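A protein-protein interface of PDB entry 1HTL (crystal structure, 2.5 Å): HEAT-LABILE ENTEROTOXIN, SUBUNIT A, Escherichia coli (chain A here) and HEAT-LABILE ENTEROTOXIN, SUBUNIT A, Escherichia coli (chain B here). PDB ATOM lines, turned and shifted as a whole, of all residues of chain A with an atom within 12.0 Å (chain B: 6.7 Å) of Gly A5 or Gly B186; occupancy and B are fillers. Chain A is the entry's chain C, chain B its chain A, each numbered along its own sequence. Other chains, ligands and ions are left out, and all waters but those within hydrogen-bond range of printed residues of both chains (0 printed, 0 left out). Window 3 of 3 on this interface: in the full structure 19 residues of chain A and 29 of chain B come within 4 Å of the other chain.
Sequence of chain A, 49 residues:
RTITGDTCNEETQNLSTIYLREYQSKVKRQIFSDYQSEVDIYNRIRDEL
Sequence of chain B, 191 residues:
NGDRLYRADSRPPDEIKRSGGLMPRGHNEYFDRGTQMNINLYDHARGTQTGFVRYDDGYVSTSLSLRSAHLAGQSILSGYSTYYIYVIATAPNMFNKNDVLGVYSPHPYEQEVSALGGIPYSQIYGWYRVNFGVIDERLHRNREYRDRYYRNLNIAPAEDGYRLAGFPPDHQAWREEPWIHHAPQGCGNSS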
ATOM      1  N   GLY A   5      22.593  29.530  -2.478  1.00  0.00           N
ATOM      2  CA  GLY A   5      24.051  29.293  -2.718  1.00  0.00           C
ATOM      3  C   GLY A   5      24.446  27.895  -2.275  1.00  0.00           C
ATOM      4  O   GLY A   5      23.725  26.930  -2.551  1.00  0.00           O
ATOM      5  N   ASP A   6      25.570  27.779  -1.570  1.00  0.00           N
ATOM      6  CA  ASP A   6      26.034  26.483  -1.070  1.00  0.00           C
ATOM      7  C   ASP A   6      24.939  25.881  -0.198  1.00  0.00           C
ATOM      8  O   ASP A   6      24.862  24.663  -0.049  1.00  0.00           O
ATOM      9  CB  ASP A   6      27.337  26.633  -0.261  1.00  0.00           C
ATOM     10  CG  ASP A   6      27.149  27.403   1.056  1.00  0.00           C
ATOM     11  OD1 ASP A   6      26.308  28.335   1.118  1.00  0.00           O
ATOM     12  OD2 ASP A   6      27.864  27.079   2.034  1.00  0.00           O
ATOM     13  N   THR A   7      24.103  26.757   0.369  1.00  0.00           N
ATOM     14  CA  THR A   7      22.974  26.373   1.212  1.00  0.00           C
ATOM     15  C   THR A   7      22.231  25.239   0.517  1.00  0.00           C
ATOM     16  O   THR A   7      21.793  24.294   1.159  1.00  0.00           O
ATOM     17  CB  THR A   7      22.020  27.572   1.430  1.00  0.00           C
ATOM     18  OG1 THR A   7      22.781  28.689   1.906  1.00  0.00           O
ATOM     19  CG2 THR A   7      20.952  27.246   2.459  1.00  0.00           C
ATOM     20  N   CYS A   8      22.180  25.308  -0.809  1.00  0.00           N
ATOM     21  CA  CYS A   8      21.531  24.282  -1.597  1.00  0.00           C
ATOM     22  C   CYS A   8      22.297  22.982  -1.353  1.00  0.00           C
ATOM     23  O   CYS A   8      21.840  22.138  -0.598  1.00  0.00           O
ATOM     24  CB  CYS A   8      21.556  24.663  -3.076  1.00  0.00           C
ATOM     25  SG  CYS A   8      20.399  23.705  -4.083  1.00  0.00           S
ATOM     26  N   ASN A   9      23.521  22.893  -1.873  1.00  0.00           N
ATOM     27  CA  ASN A   9      24.354  21.696  -1.720  1.00  0.00           C
ATOM     28  C   ASN A   9      24.639  21.309  -0.270  1.00  0.00           C
ATOM     29  O   ASN A   9      25.064  20.186   0.000  1.00  0.00           O
ATOM     30  CB  ASN A   9      25.661  21.847  -2.507  1.00  0.00           C
ATOM     31  CG  ASN A   9      25.422  22.064  -4.000  1.00  0.00           C
ATOM     32  OD1 ASN A   9      25.852  23.063  -4.569  1.00  0.00           O
ATOM     33  ND2 ASN A   9      24.710  21.139  -4.630  1.00  0.00           N
ATOM     34  N   GLU A  10      24.383  22.226   0.657  1.00  0.00           N
ATOM     35  CA  GLU A  10      24.588  21.964   2.071  1.00  0.00           C
ATOM     36  C   GLU A  10      23.264  21.507   2.665  1.00  0.00           C
ATOM     37  O   GLU A  10      23.226  20.807   3.669  1.00  0.00           O
ATOM     38  CB  GLU A  10      25.092  23.211   2.809  1.00  0.00           C
ATOM     39  CG  GLU A  10      26.145  22.876   3.900  1.00  0.00           C
ATOM     40  CD  GLU A  10      26.619  24.073   4.748  1.00  0.00           C
ATOM     41  OE1 GLU A  10      26.028  25.172   4.634  1.00  0.00           O
ATOM     42  OE2 GLU A  10      27.583  23.897   5.543  1.00  0.00           O
ATOM     43  N   GLU A  11      22.177  21.910   2.028  1.00  0.00           N
ATOM     44  CA  GLU A  11      20.840  21.533   2.462  1.00  0.00           C
ATOM     45  C   GLU A  11      20.582  20.132   1.928  1.00  0.00           C
ATOM     46  O   GLU A  11      20.011  19.285   2.609  1.00  0.00           O
ATOM     47  CB  GLU A  11      19.800  22.502   1.883  1.00  0.00           C
ATOM     48  CG  GLU A  11      18.595  22.746   2.777  1.00  0.00           C
ATOM     49  CD  GLU A  11      18.955  23.301   4.149  1.00  0.00           C
ATOM     50  OE1 GLU A  11      20.065  23.855   4.340  1.00  0.00           O
ATOM     51  OE2 GLU A  11      18.110  23.183   5.053  1.00  0.00           O
ATOM     52  N   THR A  12      21.019  19.912   0.696  1.00  0.00           N
ATOM     53  CA  THR A  12      20.885  18.648  -0.002  1.00  0.00           C
ATOM     54  C   THR A  12      21.623  17.581   0.800  1.00  0.00           C
ATOM     55  O   THR A  12      21.020  16.634   1.298  1.00  0.00           O
ATOM     56  CB  THR A  12      21.475  18.787  -1.419  1.00  0.00           C
ATOM     57  OG1 THR A  12      20.662  19.695  -2.173  1.00  0.00           O
ATOM     58  CG2 THR A  12      21.549  17.444  -2.128  1.00  0.00           C
ATOM     59  N   GLN A  13      22.906  17.824   1.038  1.00  0.00           N
ATOM     60  CA  GLN A  13      23.721  16.892   1.793  1.00  0.00           C
ATOM     61  C   GLN A  13      23.162  16.645   3.192  1.00  0.00           C
ATOM     62  O   GLN A  13      23.360  15.573   3.756  1.00  0.00           O
ATOM     63  CB  GLN A  13      25.161  17.392   1.877  1.00  0.00           C
ATOM     64  CG  GLN A  13      26.154  16.442   1.235  1.00  0.00           C
ATOM     65  CD  GLN A  13      27.183  15.892   2.231  1.00  0.00           C
ATOM     66  OE1 GLN A  13      28.321  16.362   2.288  1.00  0.00           O
ATOM     67  NE2 GLN A  13      26.790  14.888   3.003  1.00  0.00           N
ATOM     68  N   ASN A  14      22.392  17.596   3.706  1.00  0.00           N
ATOM     69  CA  ASN A  14      21.818  17.498   5.050  1.00  0.00           C
ATOM     70  C   ASN A  14      20.480  16.756   5.156  1.00  0.00           C
ATOM     71  O   ASN A  14      20.190  16.108   6.165  1.00  0.00           O
ATOM     72  CB  ASN A  14      21.681  18.898   5.646  1.00  0.00           C
ATOM     73  CG  ASN A  14      21.362  18.872   7.125  1.00  0.00           C
ATOM     74  OD1 ASN A  14      22.012  18.165   7.903  1.00  0.00           O
ATOM     75  ND2 ASN A  14      20.372  19.667   7.533  1.00  0.00           N
ATOM     76  N   LEU A  15      19.637  16.900   4.149  1.00  0.00           N
ATOM     77  CA  LEU A  15      18.353  16.222   4.156  1.00  0.00           C
ATOM     78  C   LEU A  15      18.659  14.783   3.807  1.00  0.00           C
ATOM     79  O   LEU A  15      18.007  13.860   4.277  1.00  0.00           O
ATOM     80  CB  LEU A  15      17.425  16.843   3.120  1.00  0.00           C
ATOM     81  CG  LEU A  15      17.297  18.355   3.318  1.00  0.00           C
ATOM     82  CD1 LEU A  15      16.432  18.932   2.218  1.00  0.00           C
ATOM     83  CD2 LEU A  15      16.707  18.642   4.687  1.00  0.00           C
ATOM     84  N   PRO B 168      21.742  21.590  -8.655  1.00  0.00           N
ATOM     85  CA  PRO B 168      22.399  22.757  -8.055  1.00  0.00           C
ATOM     86  C   PRO B 168      21.397  23.922  -8.010  1.00  0.00           C
ATOM     87  O   PRO B 168      20.351  23.858  -8.653  1.00  0.00           O
ATOM     88  CB  PRO B 168      23.572  23.011  -9.010  1.00  0.00           C
ATOM     89  CG  PRO B 168      23.045  22.551 -10.335  1.00  0.00           C
ATOM     90  CD  PRO B 168      22.295  21.289  -9.993  1.00  0.00           C
ATOM     91  N   PRO B 169      21.701  24.996  -7.268  1.00  0.00           N
ATOM     92  CA  PRO B 169      20.803  26.159  -7.156  1.00  0.00           C
ATOM     93  C   PRO B 169      20.267  26.779  -8.453  1.00  0.00           C
ATOM     94  O   PRO B 169      19.072  26.981  -8.602  1.00  0.00           O
ATOM     95  CB  PRO B 169      21.632  27.167  -6.339  1.00  0.00           C
ATOM     96  CG  PRO B 169      23.067  26.730  -6.566  1.00  0.00           C
ATOM     97  CD  PRO B 169      22.941  25.225  -6.505  1.00  0.00           C
ATOM     98  N   ASP B 170      21.142  27.078  -9.398  1.00  0.00           N
ATOM     99  CA  ASP B 170      20.677  27.679 -10.631  1.00  0.00           C
ATOM    100  C   ASP B 170      19.855  26.755 -11.520  1.00  0.00           C
ATOM    101  O   ASP B 170      19.190  27.223 -12.435  1.00  0.00           O
ATOM    102  CB  ASP B 170      21.830  28.328 -11.423  1.00  0.00           C
ATOM    103  CG  ASP B 170      23.159  27.562 -11.326  1.00  0.00           C
ATOM    104  OD1 ASP B 170      23.184  26.344 -11.063  1.00  0.00           O
ATOM    105  OD2 ASP B 170      24.205  28.214 -11.521  1.00  0.00           O
ATOM    106  N   ALA B 183      11.715  22.118  -2.788  1.00  0.00           N
ATOM    107  CA  ALA B 183      13.063  22.686  -2.883  1.00  0.00           C
ATOM    108  C   ALA B 183      13.659  23.123  -1.536  1.00  0.00           C
ATOM    109  O   ALA B 183      13.039  23.879  -0.785  1.00  0.00           O
ATOM    110  CB  ALA B 183      13.077  23.858  -3.874  1.00  0.00           C
ATOM    111  N   PRO B 184      14.861  22.616  -1.200  1.00  0.00           N
ATOM    112  CA  PRO B 184      15.517  22.977   0.063  1.00  0.00           C
ATOM    113  C   PRO B 184      15.777  24.494   0.141  1.00  0.00           C
ATOM    114  O   PRO B 184      15.545  25.221  -0.829  1.00  0.00           O
ATOM    115  CB  PRO B 184      16.830  22.177  -0.001  1.00  0.00           C
ATOM    116  CG  PRO B 184      16.480  20.977  -0.833  1.00  0.00           C
ATOM    117  CD  PRO B 184      15.646  21.596  -1.927  1.00  0.00           C
ATOM    118  N   GLN B 185      16.262  24.964   1.290  1.00  0.00           N
ATOM    119  CA  GLN B 185      16.555  26.383   1.485  1.00  0.00           C
ATOM    120  C   GLN B 185      17.814  26.745   0.704  1.00  0.00           C
ATOM    121  O   GLN B 185      18.838  26.092   0.839  1.00  0.00           O
ATOM    122  CB  GLN B 185      16.762  26.696   2.975  1.00  0.00           C
ATOM    123  CG  GLN B 185      15.508  26.580   3.860  1.00  0.00           C
ATOM    124  CD  GLN B 185      14.651  27.847   3.880  1.00  0.00           C
ATOM    125  OE1 GLN B 185      13.532  27.861   3.376  1.00  0.00           O
ATOM    126  NE2 GLN B 185      15.173  28.908   4.483  1.00  0.00           N
ATOM    127  N   GLY B 186      17.732  27.769  -0.134  1.00  0.00           N
ATOM    128  CA  GLY B 186      18.891  28.170  -0.910  1.00  0.00           C
ATOM    129  C   GLY B 186      18.907  27.630  -2.328  1.00  0.00           C
ATOM    130  O   GLY B 186      19.816  27.965  -3.101  1.00  0.00           O
ATOM    131  N   CYS B 187      17.924  26.793  -2.660  1.00  0.00           N
ATOM    132  CA  CYS B 187      17.798  26.197  -3.992  1.00  0.00           C
ATOM    133  C   CYS B 187      16.641  26.846  -4.768  1.00  0.00           C
ATOM    134  O   CYS B 187      15.560  27.055  -4.208  1.00  0.00           O
ATOM    135  CB  CYS B 187      17.533  24.684  -3.891  1.00  0.00           C
ATOM    136  SG  CYS B 187      18.726  23.696  -2.937  1.00  0.00           S
ATOM    137  N   GLY B 188      16.875  27.139  -6.050  1.00  0.00           N
ATOM    138  CA  GLY B 188      15.866  27.748  -6.903  1.00  0.00           C
ATOM    139  C   GLY B 188      15.303  29.049  -6.355  1.00  0.00           C
ATOM    140  O   GLY B 188      15.937  30.115  -6.521  1.00  0.00           O
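The backbone NH (N) of Gly A5 is in hydrogen-bond range of the backbone carbonyl oxygen (O) of Gly B186, 3.2 Å away. The side-chain sulfur (SG) of Cys B187 forms a disulfide with the side-chain sulfur (SG) of Cys A8, at 2.0 Å. The backbone carbonyl oxygen (O) of Thr A7 lies close to the backbone carbonyl oxygen (O) of Gln B185 (3.5 Å). The backbone nitrogen (N) of Pro B169 lies close to the side-chain sulfur (SG) of Cys A8, at 3.7 Å.
The backbone carbonyl oxygen (O) of Pro B169 sits at hydrogen-bond distance from the backbone NH (N) of Gly B188 (3.4 Å). The side-chain hydroxyl (OG1) of Thr A12 is in hydrogen-bond range of the backbone carbonyl oxygen (O) of Cys A8 (3.1 Å).
Among the printed residues, pairs that only touch across the chains: Thr A7 with Gly B186, Cys A8 with Gln B185, Cys A8 with Gly B186, Glu A11 with Pro B184, Glu A11 with Gln B185 and Leu A15 with Pro B184.
Of chain B, only Gly B186 (3.2 Å) comes within 4 Å of Gly A5. Gly B186 touches just these residues of chain A: Gly A5, Thr A7 and Cys A8. Of chain A, only Cys A8 (3.7 Å) comes within 4 Å of Pro B169. Gln B185 touches three residues of chain A. Of chain A, only Cys A8 (2.0 Å) comes within 4 Å of Cys B187. No residue of chain A comes within 4 Å of Gly B188. Printed residues of chain B within 4 Å of Cys A8: Pro B169 (3.7 Å), Gln B185 (3.8 Å), Gly B186 (3.7 Å) and Cys B187 (2.0 Å). Of the printed residues of chain B, Glu A11 touches Pro B184 (3.3 Å) and Gln B185 (3.5 Å). Printed residues of chain B within 4 Å of Leu A15: Pro B184 (3.7 Å). Of the printed residues of chain B, Thr A7 touches Gln B185 and Gly B186. Asn A14 touches none of the printed residues of chain B. The nearest residue of chain B that does not touch Gly A5 is Pro B169 (4.1 Å). The nearest printed residue of chain B that does not touch Cys A8 is Pro B168 (4.1 Å).
Of the 11 printed residues of chain A, 5 touch a printed residue of chain B. Hydrophobic or aromatic side chains of chain A within 4 Å of the printed part of chain B: Leu A15. Of the 9 printed residues of chain B, 5 touch a printed residue of chain A. Hydrophobic or aromatic side chains of chain B within 4 Å of the printed part of chain A: Pro B169 and Pro B184. Along chain B the printed residues that touch a printed residue of chain A span positions 169 to 187.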
